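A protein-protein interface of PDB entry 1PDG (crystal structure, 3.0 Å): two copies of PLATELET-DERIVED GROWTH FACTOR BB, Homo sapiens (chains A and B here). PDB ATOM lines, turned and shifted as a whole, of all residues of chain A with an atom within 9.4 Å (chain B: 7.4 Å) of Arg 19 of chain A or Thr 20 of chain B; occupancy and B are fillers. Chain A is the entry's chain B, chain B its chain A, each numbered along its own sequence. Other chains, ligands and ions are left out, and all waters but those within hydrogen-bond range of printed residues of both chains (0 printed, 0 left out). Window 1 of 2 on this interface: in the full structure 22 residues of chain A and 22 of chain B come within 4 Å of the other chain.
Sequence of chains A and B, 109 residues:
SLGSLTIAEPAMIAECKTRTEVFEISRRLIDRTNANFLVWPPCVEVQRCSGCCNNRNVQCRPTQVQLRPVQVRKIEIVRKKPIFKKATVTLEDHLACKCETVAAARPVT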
ATOM      1  N   MET A  12     -12.621  25.136  19.020  1.00  0.00           N
ATOM      2  CA  MET A  12     -11.397  24.880  18.190  1.00  0.00           C
ATOM      3  C   MET A  12     -10.462  24.072  19.064  1.00  0.00           C
ATOM      4  O   MET A  12     -10.228  24.461  20.211  1.00  0.00           O
ATOM      5  CB  MET A  12     -10.875  26.242  17.768  1.00  0.00           C
ATOM      6  CG  MET A  12     -10.208  26.366  16.453  1.00  0.00           C
ATOM      7  SD  MET A  12     -11.163  25.448  15.193  1.00  0.00           S
ATOM      8  CE  MET A  12     -12.437  26.730  14.839  1.00  0.00           C
ATOM      9  N   ILE A  13     -10.006  22.952  18.558  1.00  0.00           N
ATOM     10  CA  ILE A  13      -9.099  22.027  19.222  1.00  0.00           C
ATOM     11  C   ILE A  13      -7.894  22.800  19.795  1.00  0.00           C
ATOM     12  O   ILE A  13      -7.396  23.717  19.111  1.00  0.00           O
ATOM     13  CB  ILE A  13      -8.482  20.960  18.217  1.00  0.00           C
ATOM     14  CG1 ILE A  13      -7.869  19.802  18.999  1.00  0.00           C
ATOM     15  CG2 ILE A  13      -7.406  21.632  17.306  1.00  0.00           C
ATOM     16  CD1 ILE A  13      -8.768  18.666  19.507  1.00  0.00           C
ATOM     17  N   ALA A  14      -7.440  22.310  20.924  1.00  0.00           N
ATOM     18  CA  ALA A  14      -6.217  22.843  21.562  1.00  0.00           C
ATOM     19  C   ALA A  14      -5.077  22.088  20.865  1.00  0.00           C
ATOM     20  O   ALA A  14      -4.646  21.062  21.391  1.00  0.00           O
ATOM     21  CB  ALA A  14      -6.271  22.535  23.033  1.00  0.00           C
ATOM     22  N   GLU A  15      -4.788  22.534  19.666  1.00  0.00           N
ATOM     23  CA  GLU A  15      -3.747  21.900  18.819  1.00  0.00           C
ATOM     24  C   GLU A  15      -2.537  21.620  19.684  1.00  0.00           C
ATOM     25  O   GLU A  15      -2.203  22.569  20.455  1.00  0.00           O
ATOM     26  CB  GLU A  15      -3.294  22.880  17.752  1.00  0.00           C
ATOM     27  CG  GLU A  15      -2.192  22.363  16.813  1.00  0.00           C
ATOM     28  CD  GLU A  15      -0.975  23.256  16.765  1.00  0.00           C
ATOM     29  OE1 GLU A  15      -1.016  24.450  17.036  1.00  0.00           O
ATOM     30  OE2 GLU A  15       0.048  22.574  16.453  1.00  0.00           O
ATOM     31  N   CYS A  16      -1.883  20.488  19.569  1.00  0.00           N
ATOM     32  CA  CYS A  16      -0.777  20.109  20.466  1.00  0.00           C
ATOM     33  C   CYS A  16       0.598  20.645  20.133  1.00  0.00           C
ATOM     34  O   CYS A  16       1.250  20.104  19.223  1.00  0.00           O
ATOM     35  CB  CYS A  16      -0.709  18.572  20.551  1.00  0.00           C
ATOM     36  SG  CYS A  16       0.912  17.930  21.055  1.00  0.00           S
ATOM     37  N   LYS A  17       1.043  21.614  20.928  1.00  0.00           N
ATOM     38  CA  LYS A  17       2.380  22.204  20.778  1.00  0.00           C
ATOM     39  C   LYS A  17       2.961  22.660  22.098  1.00  0.00           C
ATOM     40  O   LYS A  17       2.540  22.168  23.185  1.00  0.00           O
ATOM     41  CB  LYS A  17       2.516  23.161  19.641  1.00  0.00           C
ATOM     42  CG  LYS A  17       1.315  23.987  19.261  1.00  0.00           C
ATOM     43  CD  LYS A  17       1.175  25.119  20.255  1.00  0.00           C
ATOM     44  CE  LYS A  17       0.202  26.181  19.892  1.00  0.00           C
ATOM     45  NZ  LYS A  17       0.191  26.468  18.438  1.00  0.00           N
ATOM     46  N   THR A  18       4.025  23.414  22.079  1.00  0.00           N
ATOM     47  CA  THR A  18       4.740  23.920  23.286  1.00  0.00           C
ATOM     48  C   THR A  18       3.950  25.063  23.878  1.00  0.00           C
ATOM     49  O   THR A  18       3.637  26.013  23.091  1.00  0.00           O
ATOM     50  CB  THR A  18       6.153  24.369  22.739  1.00  0.00           C
ATOM     51  OG1 THR A  18       7.193  23.827  23.551  1.00  0.00           O
ATOM     52  CG2 THR A  18       6.307  25.887  22.516  1.00  0.00           C
ATOM     53  N   ARG A  19       3.604  25.064  25.136  1.00  0.00           N
ATOM     54  CA  ARG A  19       2.792  26.228  25.671  1.00  0.00           C
ATOM     55  C   ARG A  19       3.407  26.695  26.946  1.00  0.00           C
ATOM     56  O   ARG A  19       4.111  25.792  27.503  1.00  0.00           O
ATOM     57  CB  ARG A  19       1.346  25.772  25.793  1.00  0.00           C
ATOM     58  CG  ARG A  19       0.449  26.222  24.661  1.00  0.00           C
ATOM     59  CD  ARG A  19      -0.948  26.435  25.121  1.00  0.00           C
ATOM     60  NE  ARG A  19      -1.856  26.120  24.007  1.00  0.00           N
ATOM     61  CZ  ARG A  19      -1.876  24.832  23.636  1.00  0.00           C
ATOM     62  NH1 ARG A  19      -1.345  23.943  24.454  1.00  0.00           N
ATOM     63  NH2 ARG A  19      -1.967  24.568  22.350  1.00  0.00           N
ATOM     64  N   THR A  20       3.233  27.903  27.452  1.00  0.00           N
ATOM     65  CA  THR A  20       3.937  28.246  28.711  1.00  0.00           C
ATOM     66  C   THR A  20       3.143  27.813  29.930  1.00  0.00           C
ATOM     67  O   THR A  20       1.903  27.971  29.932  1.00  0.00           O
ATOM     68  CB  THR A  20       4.317  29.748  28.865  1.00  0.00           C
ATOM     69  OG1 THR A  20       4.907  30.126  27.608  1.00  0.00           O
ATOM     70  CG2 THR A  20       5.202  29.985  30.077  1.00  0.00           C
ATOM     71  N   GLU A  21       3.861  27.351  30.911  1.00  0.00           N
ATOM     72  CA  GLU A  21       3.245  26.826  32.153  1.00  0.00           C
ATOM     73  C   GLU A  21       3.924  27.479  33.339  1.00  0.00           C
ATOM     74  O   GLU A  21       5.122  27.764  33.145  1.00  0.00           O
ATOM     75  CB  GLU A  21       3.523  25.322  32.263  1.00  0.00           C
ATOM     76  CG  GLU A  21       3.302  24.372  31.109  1.00  0.00           C
ATOM     77  CD  GLU A  21       2.228  23.332  31.279  1.00  0.00           C
ATOM     78  OE1 GLU A  21       2.017  23.202  32.522  1.00  0.00           O
ATOM     79  OE2 GLU A  21       1.655  22.693  30.374  1.00  0.00           O
ATOM     80  N   VAL A  22       3.299  27.667  34.482  1.00  0.00           N
ATOM     81  CA  VAL A  22       4.011  28.321  35.604  1.00  0.00           C
ATOM     82  C   VAL A  22       4.382  27.303  36.659  1.00  0.00           C
ATOM     83  O   VAL A  22       3.482  26.895  37.415  1.00  0.00           O
ATOM     84  CB  VAL A  22       3.155  29.478  36.140  1.00  0.00           C
ATOM     85  CG1 VAL A  22       3.722  30.017  37.441  1.00  0.00           C
ATOM     86  CG2 VAL A  22       2.972  30.589  35.129  1.00  0.00           C
ATOM     87  N   GLU A  45       8.748  30.289  34.711  1.00  0.00           N
ATOM     88  CA  GLU A  45       8.108  29.928  33.448  1.00  0.00           C
ATOM     89  C   GLU A  45       8.848  28.819  32.744  1.00  0.00           C
ATOM     90  O   GLU A  45      10.066  29.003  32.491  1.00  0.00           O
ATOM     91  CB  GLU A  45       8.084  31.130  32.481  1.00  0.00           C
ATOM     92  CG  GLU A  45       7.163  32.256  32.768  1.00  0.00           C
ATOM     93  CD  GLU A  45       7.245  33.569  32.109  1.00  0.00           C
ATOM     94  OE1 GLU A  45       7.998  34.527  32.309  1.00  0.00           O
ATOM     95  OE2 GLU A  45       6.324  33.692  31.252  1.00  0.00           O
ATOM     96  N   VAL A  46       8.227  27.724  32.405  1.00  0.00           N
ATOM     97  CA  VAL A  46       8.860  26.601  31.720  1.00  0.00           C
ATOM     98  C   VAL A  46       7.856  25.992  30.737  1.00  0.00           C
ATOM     99  O   VAL A  46       6.708  25.820  31.110  1.00  0.00           O
ATOM    100  CB  VAL A  46       9.445  25.566  32.674  1.00  0.00           C
ATOM    101  CG1 VAL A  46       8.871  25.659  34.077  1.00  0.00           C
ATOM    102  CG2 VAL A  46       9.245  24.156  32.112  1.00  0.00           C
ATOM    103  N   GLN A  47       8.372  25.622  29.590  1.00  0.00           N
ATOM    104  CA  GLN A  47       7.626  25.055  28.469  1.00  0.00           C
ATOM    105  C   GLN A  47       7.173  23.641  28.710  1.00  0.00           C
ATOM    106  O   GLN A  47       7.841  22.936  29.508  1.00  0.00           O
ATOM    107  CB  GLN A  47       8.442  25.180  27.174  1.00  0.00           C
ATOM    108  CG  GLN A  47       7.947  26.367  26.345  1.00  0.00           C
ATOM    109  CD  GLN A  47       8.849  26.649  25.178  1.00  0.00           C
ATOM    110  OE1 GLN A  47       8.550  26.535  23.988  1.00  0.00           O
ATOM    111  NE2 GLN A  47      10.072  27.029  25.607  1.00  0.00           N
ATOM    112  N   ARG A  48       6.095  23.223  28.118  1.00  0.00           N
ATOM    113  CA  ARG A  48       5.568  21.868  28.351  1.00  0.00           C
ATOM    114  C   ARG A  48       4.473  21.608  27.312  1.00  0.00           C
ATOM    115  O   ARG A  48       3.774  22.563  26.901  1.00  0.00           O
ATOM    116  CB  ARG A  48       5.022  21.699  29.752  1.00  0.00           C
ATOM    117  CG  ARG A  48       5.857  21.708  30.967  1.00  0.00           C
ATOM    118  CD  ARG A  48       6.573  20.496  31.365  1.00  0.00           C
ATOM    119  NE  ARG A  48       7.313  20.541  32.607  1.00  0.00           N
ATOM    120  CZ  ARG A  48       6.914  21.071  33.768  1.00  0.00           C
ATOM    121  NH1 ARG A  48       5.776  21.763  33.965  1.00  0.00           N
ATOM    122  NH2 ARG A  48       7.615  20.853  34.906  1.00  0.00           N
ATOM    123  N   CYS A  49       4.434  20.362  26.865  1.00  0.00           N
ATOM    124  CA  CYS A  49       3.420  19.960  25.852  1.00  0.00           C
ATOM    125  C   CYS A  49       2.114  19.975  26.642  1.00  0.00           C
ATOM    126  O   CYS A  49       2.134  19.589  27.822  1.00  0.00           O
ATOM    127  CB  CYS A  49       3.795  18.626  25.294  1.00  0.00           C
ATOM    128  SG  CYS A  49       5.451  18.634  24.573  1.00  0.00           S
ATOM    129  N   SER A  50       1.147  20.578  26.046  1.00  0.00           N
ATOM    130  CA  SER A  50      -0.215  20.795  26.578  1.00  0.00           C
ATOM    131  C   SER A  50      -1.056  20.604  25.312  1.00  0.00           C
ATOM    132  O   SER A  50      -0.468  20.958  24.242  1.00  0.00           O
ATOM    133  CB  SER A  50      -0.378  22.203  27.107  1.00  0.00           C
ATOM    134  OG  SER A  50       0.625  22.733  27.990  1.00  0.00           O
ATOM    135  N   GLY A  51      -2.207  19.978  25.381  1.00  0.00           N
ATOM    136  CA  GLY A  51      -2.961  19.806  24.092  1.00  0.00           C
ATOM    137  C   GLY A  51      -3.549  18.418  23.952  1.00  0.00           C
ATOM    138  O   GLY A  51      -3.296  17.511  24.766  1.00  0.00           O
ATOM    139  N   CYS A  52      -4.344  18.260  22.887  1.00  0.00           N
ATOM    140  CA  CYS A  52      -5.126  17.075  22.615  1.00  0.00           C
ATOM    141  C   CYS A  52      -4.893  16.439  21.242  1.00  0.00           C
ATOM    142  O   CYS A  52      -4.692  17.088  20.213  1.00  0.00           O
ATOM    143  CB  CYS A  52      -6.620  17.466  22.650  1.00  0.00           C
ATOM    144  SG  CYS A  52      -6.958  19.045  23.500  1.00  0.00           S
ATOM    145  N   CYS A  60      -0.779  13.156  23.255  1.00  0.00           N
ATOM    146  CA  CYS A  60       0.187  14.217  22.884  1.00  0.00           C
ATOM    147  C   CYS A  60       1.285  14.375  23.946  1.00  0.00           C
ATOM    148  O   CYS A  60       1.064  14.843  25.066  1.00  0.00           O
ATOM    149  CB  CYS A  60      -0.435  15.530  22.459  1.00  0.00           C
ATOM    150  SG  CYS A  60       0.470  17.050  22.849  1.00  0.00           S
ATOM    151  N   GLU A  92      13.117  21.582  33.214  1.00  0.00           N
ATOM    152  CA  GLU A  92      12.875  20.714  32.054  1.00  0.00           C
ATOM    153  C   GLU A  92      11.921  21.460  31.114  1.00  0.00           C
ATOM    154  O   GLU A  92      10.742  21.675  31.474  1.00  0.00           O
ATOM    155  CB  GLU A  92      12.276  19.380  32.382  1.00  0.00           C
ATOM    156  CG  GLU A  92      12.398  18.277  31.306  1.00  0.00           C
ATOM    157  CD  GLU A  92      11.707  16.991  31.743  1.00  0.00           C
ATOM    158  OE1 GLU A  92      12.508  16.359  32.495  1.00  0.00           O
ATOM    159  OE2 GLU A  92      10.544  16.696  31.463  1.00  0.00           O
ATOM    160  N   ASP A  93      12.502  21.851  29.986  1.00  0.00           N
ATOM    161  CA  ASP A  93      11.709  22.573  28.959  1.00  0.00           C
ATOM    162  C   ASP A  93      11.204  21.520  28.007  1.00  0.00           C
ATOM    163  O   ASP A  93      11.524  20.350  28.285  1.00  0.00           O
ATOM    164  CB  ASP A  93      12.446  23.773  28.422  1.00  0.00           C
ATOM    165  CG  ASP A  93      12.257  24.926  29.420  1.00  0.00           C
ATOM    166  OD1 ASP A  93      11.611  24.734  30.469  1.00  0.00           O
ATOM    167  OD2 ASP A  93      12.813  25.978  29.144  1.00  0.00           O
ATOM    168  N   HIS A  94      10.414  21.849  27.039  1.00  0.00           N
ATOM    169  CA  HIS A  94       9.848  20.913  26.050  1.00  0.00           C
ATOM    170  C   HIS A  94       9.974  21.656  24.730  1.00  0.00           C
ATOM    171  O   HIS A  94       9.186  22.606  24.516  1.00  0.00           O
ATOM    172  CB  HIS A  94       8.386  20.620  26.413  1.00  0.00           C
ATOM    173  CG  HIS A  94       8.161  19.681  27.552  1.00  0.00           C
ATOM    174  ND1 HIS A  94       8.112  18.313  27.486  1.00  0.00           N
ATOM    175  CD2 HIS A  94       7.884  19.947  28.849  1.00  0.00           C
ATOM    176  CE1 HIS A  94       7.883  17.787  28.668  1.00  0.00           C
ATOM    177  NE2 HIS A  94       7.719  18.747  29.521  1.00  0.00           N
ATOM    178  N   LEU A  95      10.995  21.386  23.952  1.00  0.00           N
ATOM    179  CA  LEU A  95      11.286  22.061  22.712  1.00  0.00           C
ATOM    180  C   LEU A  95      10.393  21.815  21.526  1.00  0.00           C
ATOM    181  O   LEU A  95      10.511  22.645  20.571  1.00  0.00           O
ATOM    182  CB  LEU A  95      12.745  21.786  22.267  1.00  0.00           C
ATOM    183  CG  LEU A  95      13.795  22.259  23.252  1.00  0.00           C
ATOM    184  CD1 LEU A  95      15.191  21.893  22.729  1.00  0.00           C
ATOM    185  CD2 LEU A  95      13.654  23.770  23.400  1.00  0.00           C
ATOM    186  N   ALA A  96       9.754  20.679  21.422  1.00  0.00           N
ATOM    187  CA  ALA A  96       8.912  20.427  20.208  1.00  0.00           C
ATOM    188  C   ALA A  96       8.163  19.127  20.406  1.00  0.00           C
ATOM    189  O   ALA A  96       8.839  18.104  20.398  1.00  0.00           O
ATOM    190  CB  ALA A  96       9.832  20.358  18.994  1.00  0.00           C
ATOM    191  N   CYS A  97       6.869  19.218  20.514  1.00  0.00           N
ATOM    192  CA  CYS A  97       5.990  18.081  20.748  1.00  0.00           C
ATOM    193  C   CYS A  97       5.330  17.489  19.477  1.00  0.00           C
ATOM    194  O   CYS A  97       5.266  18.080  18.405  1.00  0.00           O
ATOM    195  CB  CYS A  97       4.878  18.521  21.681  1.00  0.00           C
ATOM    196  SG  CYS A  97       5.257  19.748  22.888  1.00  0.00           S
ATOM    197  N   THR B  18      -1.885  36.765  32.354  1.00  0.00           N
ATOM    198  CA  THR B  18      -2.634  35.674  31.795  1.00  0.00           C
ATOM    199  C   THR B  18      -1.997  34.980  30.598  1.00  0.00           C
ATOM    200  O   THR B  18      -1.892  35.563  29.522  1.00  0.00           O
ATOM    201  CB  THR B  18      -4.027  36.185  31.227  1.00  0.00           C
ATOM    202  OG1 THR B  18      -3.659  36.977  30.088  1.00  0.00           O
ATOM    203  CG2 THR B  18      -4.831  36.930  32.244  1.00  0.00           C
ATOM    204  N   ARG B  19      -1.755  33.718  30.709  1.00  0.00           N
ATOM    205  CA  ARG B  19      -1.175  32.806  29.743  1.00  0.00           C
ATOM    206  C   ARG B  19      -2.253  31.747  29.410  1.00  0.00           C
ATOM    207  O   ARG B  19      -2.855  31.245  30.374  1.00  0.00           O
ATOM    208  CB  ARG B  19       0.007  32.031  30.306  1.00  0.00           C
ATOM    209  CG  ARG B  19       0.820  32.518  31.456  1.00  0.00           C
ATOM    210  CD  ARG B  19       2.246  32.324  31.214  1.00  0.00           C
ATOM    211  NE  ARG B  19       3.179  32.641  32.229  1.00  0.00           N
ATOM    212  CZ  ARG B  19       2.975  33.609  33.111  1.00  0.00           C
ATOM    213  NH1 ARG B  19       1.810  34.216  32.966  1.00  0.00           N
ATOM    214  NH2 ARG B  19       3.844  33.914  34.057  1.00  0.00           N
ATOM    215  N   THR B  20      -2.343  31.365  28.160  1.00  0.00           N
ATOM    216  CA  THR B  20      -3.326  30.382  27.734  1.00  0.00           C
ATOM    217  C   THR B  20      -3.014  29.015  28.333  1.00  0.00           C
ATOM    218  O   THR B  20      -1.884  28.730  28.679  1.00  0.00           O
ATOM    219  CB  THR B  20      -3.540  30.281  26.193  1.00  0.00           C
ATOM    220  OG1 THR B  20      -2.705  29.209  25.748  1.00  0.00           O
ATOM    221  CG2 THR B  20      -3.355  31.578  25.444  1.00  0.00           C
ATOM    222  N   GLU B  21      -4.081  28.272  28.498  1.00  0.00           N
ATOM    223  CA  GLU B  21      -4.049  26.928  29.059  1.00  0.00           C
ATOM    224  C   GLU B  21      -4.978  26.069  28.210  1.00  0.00           C
ATOM    225  O   GLU B  21      -5.770  26.667  27.448  1.00  0.00           O
ATOM    226  CB  GLU B  21      -4.517  26.845  30.486  1.00  0.00           C
ATOM    227  CG  GLU B  21      -4.526  28.001  31.422  1.00  0.00           C
ATOM    228  CD  GLU B  21      -4.184  27.925  32.873  1.00  0.00           C
ATOM    229  OE1 GLU B  21      -4.971  27.300  33.634  1.00  0.00           O
ATOM    230  OE2 GLU B  21      -3.203  28.568  33.302  1.00  0.00           O
ATOM    231  N   VAL B  22      -4.813  24.774  28.263  1.00  0.00           N
ATOM    232  CA  VAL B  22      -5.776  23.895  27.528  1.00  0.00           C
ATOM    233  C   VAL B  22      -6.661  23.354  28.652  1.00  0.00           C
ATOM    234  O   VAL B  22      -6.127  23.197  29.741  1.00  0.00           O
ATOM    235  CB  VAL B  22      -5.037  22.912  26.688  1.00  0.00           C
ATOM    236  CG1 VAL B  22      -3.581  23.269  26.459  1.00  0.00           C
ATOM    237  CG2 VAL B  22      -5.198  21.487  27.189  1.00  0.00           C
ATOM    238  N   VAL B  44     -10.306  22.605  24.079  1.00  0.00           N
ATOM    239  CA  VAL B  44     -10.139  23.970  23.632  1.00  0.00           C
ATOM    240  C   VAL B  44      -9.116  24.725  24.447  1.00  0.00           C
ATOM    241  O   VAL B  44      -8.847  24.313  25.609  1.00  0.00           O
ATOM    242  CB  VAL B  44     -11.579  24.575  23.850  1.00  0.00           C
ATOM    243  CG1 VAL B  44     -12.434  24.126  22.666  1.00  0.00           C
ATOM    244  CG2 VAL B  44     -12.241  24.136  25.134  1.00  0.00           C
ATOM    245  N   GLU B  45      -8.543  25.803  23.935  1.00  0.00           N
ATOM    246  CA  GLU B  45      -7.617  26.609  24.777  1.00  0.00           C
ATOM    247  C   GLU B  45      -8.480  27.821  25.245  1.00  0.00           C
ATOM    248  O   GLU B  45      -9.168  28.405  24.404  1.00  0.00           O
ATOM    249  CB  GLU B  45      -6.464  27.183  24.147  1.00  0.00           C
ATOM    250  CG  GLU B  45      -5.238  26.714  23.487  1.00  0.00           C
ATOM    251  CD  GLU B  45      -5.011  27.368  22.140  1.00  0.00           C
ATOM    252  OE1 GLU B  45      -6.043  28.033  21.788  1.00  0.00           O
ATOM    253  OE2 GLU B  45      -4.048  27.231  21.414  1.00  0.00           O
ATOM    254  N   VAL B  46      -8.426  28.060  26.512  1.00  0.00           N
ATOM    255  CA  VAL B  46      -9.086  29.180  27.199  1.00  0.00           C
ATOM    256  C   VAL B  46      -7.943  29.979  27.859  1.00  0.00           C
ATOM    257  O   VAL B  46      -6.895  29.322  28.130  1.00  0.00           O
ATOM    258  CB  VAL B  46     -10.107  28.710  28.255  1.00  0.00           C
ATOM    259  CG1 VAL B  46     -11.270  27.941  27.661  1.00  0.00           C
ATOM    260  CG2 VAL B  46      -9.527  28.001  29.447  1.00  0.00           C
ATOM    261  N   GLN B  47      -8.168  31.231  28.201  1.00  0.00           N
ATOM    262  CA  GLN B  47      -7.098  32.012  28.849  1.00  0.00           C
ATOM    263  C   GLN B  47      -7.259  32.218  30.325  1.00  0.00           C
ATOM    264  O   GLN B  47      -8.119  32.985  30.729  1.00  0.00           O
ATOM    265  CB  GLN B  47      -6.871  33.300  28.114  1.00  0.00           C
ATOM    266  CG  GLN B  47      -5.747  33.136  27.034  1.00  0.00           C
ATOM    267  CD  GLN B  47      -4.951  34.432  27.123  1.00  0.00           C
ATOM    268  OE1 GLN B  47      -5.532  35.443  27.584  1.00  0.00           O
ATOM    269  NE2 GLN B  47      -3.679  34.354  26.865  1.00  0.00           N
ATOM    270  N   ARG B  48      -6.377  31.751  31.135  1.00  0.00           N
ATOM    271  CA  ARG B  48      -6.231  31.763  32.537  1.00  0.00           C
ATOM    272  C   ARG B  48      -5.060  32.528  33.131  1.00  0.00           C
ATOM    273  O   ARG B  48      -3.950  32.388  32.652  1.00  0.00           O
ATOM    274  CB  ARG B  48      -5.955  30.289  32.984  1.00  0.00           C
ATOM    275  CG  ARG B  48      -6.982  29.732  33.923  1.00  0.00           C
ATOM    276  CD  ARG B  48      -8.317  30.341  33.854  1.00  0.00           C
ATOM    277  NE  ARG B  48      -9.202  29.738  32.840  1.00  0.00           N
ATOM    278  CZ  ARG B  48     -10.393  29.287  33.286  1.00  0.00           C
ATOM    279  NH1 ARG B  48     -10.640  29.244  34.612  1.00  0.00           N
ATOM    280  NH2 ARG B  48     -11.397  29.199  32.412  1.00  0.00           N
ATOM    281  N   CYS B  49      -5.274  33.069  34.310  1.00  0.00           N
ATOM    282  CA  CYS B  49      -4.395  33.837  35.155  1.00  0.00           C
ATOM    283  C   CYS B  49      -3.399  33.008  35.973  1.00  0.00           C
ATOM    284  O   CYS B  49      -3.855  32.456  36.998  1.00  0.00           O
ATOM    285  CB  CYS B  49      -5.229  34.561  36.228  1.00  0.00           C
ATOM    286  SG  CYS B  49      -5.735  36.168  35.929  1.00  0.00           S
ATOM    287  N   SER B  50      -2.136  33.102  35.667  1.00  0.00           N
ATOM    288  CA  SER B  50      -1.080  32.336  36.320  1.00  0.00           C
ATOM    289  C   SER B  50       0.127  33.207  36.602  1.00  0.00           C
ATOM    290  O   SER B  50       0.482  33.959  35.687  1.00  0.00           O
ATOM    291  CB  SER B  50      -0.627  31.280  35.277  1.00  0.00           C
ATOM    292  OG  SER B  50       0.135  31.873  34.257  1.00  0.00           O
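The guanidinium group (NH2) of Arg 19 of chain A is in salt-bridge range of the side-chain carboxylate (OE2) of Glu 45 of chain B (3.5 Å).
The guanidinium group (NE) of Arg 19 of chain B lies within salt-bridge range of the side-chain carboxylate (OE2) of Glu 45 of chain A.
The backbone carbonyl oxygen (O) of Ser 50 of chain B lies within hydrogen-bond range of the guanidinium group (NH1) of Arg 19 of chain B.
The side-chain sulfur (SG) of Cys 60 of chain A is disulfide-bonded to the side-chain sulfur (SG) of Cys 16 of chain A (2.0 Å).
N of Cys 52 of chain A is in hydrogen-bond range of O of Ala 14 of chain A (3.2 Å).
The backbone carbonyl oxygen (O) of Arg 48 of chain A is in hydrogen-bond range of the side-chain hydroxyl (OG) of Ser 50 of chain A, at 3.3 Å.
SG of Cys 97 of chain A forms a disulfide with SG of Cys 49 of chain A, at 2.0 Å.
The backbone carbonyl oxygen (O) of Glu 15 of chain A is in hydrogen-bond range of the guanidinium group (NH2) of Arg 19 of chain A (2.8 Å).
Among the printed residues, pairs that only touch across the chains: Arg 19 of chain A with Val 22 of chain B (3.1 Å), Val 22 of chain A with Ser 50 of chain B (3.2 Å), Met 12 of chain A with Val 44 of chain B (3.3 Å), Arg 19 of chain A with Thr 20 of chain B (3.3 Å), Ser 50 of chain A with Val 22 of chain B (3.4 Å), Val 22 of chain A with Arg 19 of chain B (3.6 Å), Gly 51 of chain A with Val 22 of chain B (3.7 Å), Ala 14 of chain A with Val 44 of chain B (3.9 Å), Ala 14 of chain A with Val 22 of chain B (3.9 Å) and Thr 20 of chain A with Arg 19 of chain B (3.9 Å).
Arg 19 of chain A touches three residues of chain B.
Printed residues of chain B within 4 Å of Thr 20 of chain A: Arg 19.
Of the printed residues of chain B, Val 22 of chain A touches Arg 19 and Ser 50.
Of the printed residues of chain B, Glu 45 of chain A touches Arg 19.
Of the printed residues of chain B, Ser 50 of chain A touches Val 22 (3.4 Å).
Of chain A, only Arg 19 comes within 4 Å of Thr 20 of chain B.
Gln 47 of chain B touches none of the printed residues of chain A.
Of the printed residues of chain A, Ser 50 of chain B touches Val 22.
The nearest residue of chain A that does not touch Thr 20 of chain B is Thr 20 of chain A (4.1 Å).
Of the 26 printed residues of chain A, 8 touch a printed residue of chain B.
Of the 12 printed residues of chain B, 6 touch a printed residue of chain A.
Hydrophobic or aromatic side chains of chain B that line the printed part of chain A: Val 22 and Val 44.
Among the printed residues, 12 pairs touch across the chains.
Among the printed residues, Asp or Glu carboxylates within 4 Å of a Lys or Arg side-chain nitrogen of the other chain: Arg 19 of chain A with Glu 45 of chain B and Glu 45 of chain A with Arg 19 of chain B.
Arg 19 of chain A touches Thr 20 of chain B, and with the chains exchanged Thr 20 of chain A touches Arg 19 of chain B.
Arg 19 of chain A touches Val 22 of chain B, and with the chains exchanged Val 22 of chain A touches Arg 19 of chain B.
Arg 19 of chain A touches Glu 45 of chain B, and with the chains exchanged Glu 45 of chain A touches Arg 19 of chain B.
Val 22 of chain A touches Ser 50 of chain B, and with the chains exchanged Ser 50 of chain A touches Val 22 of chain B.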
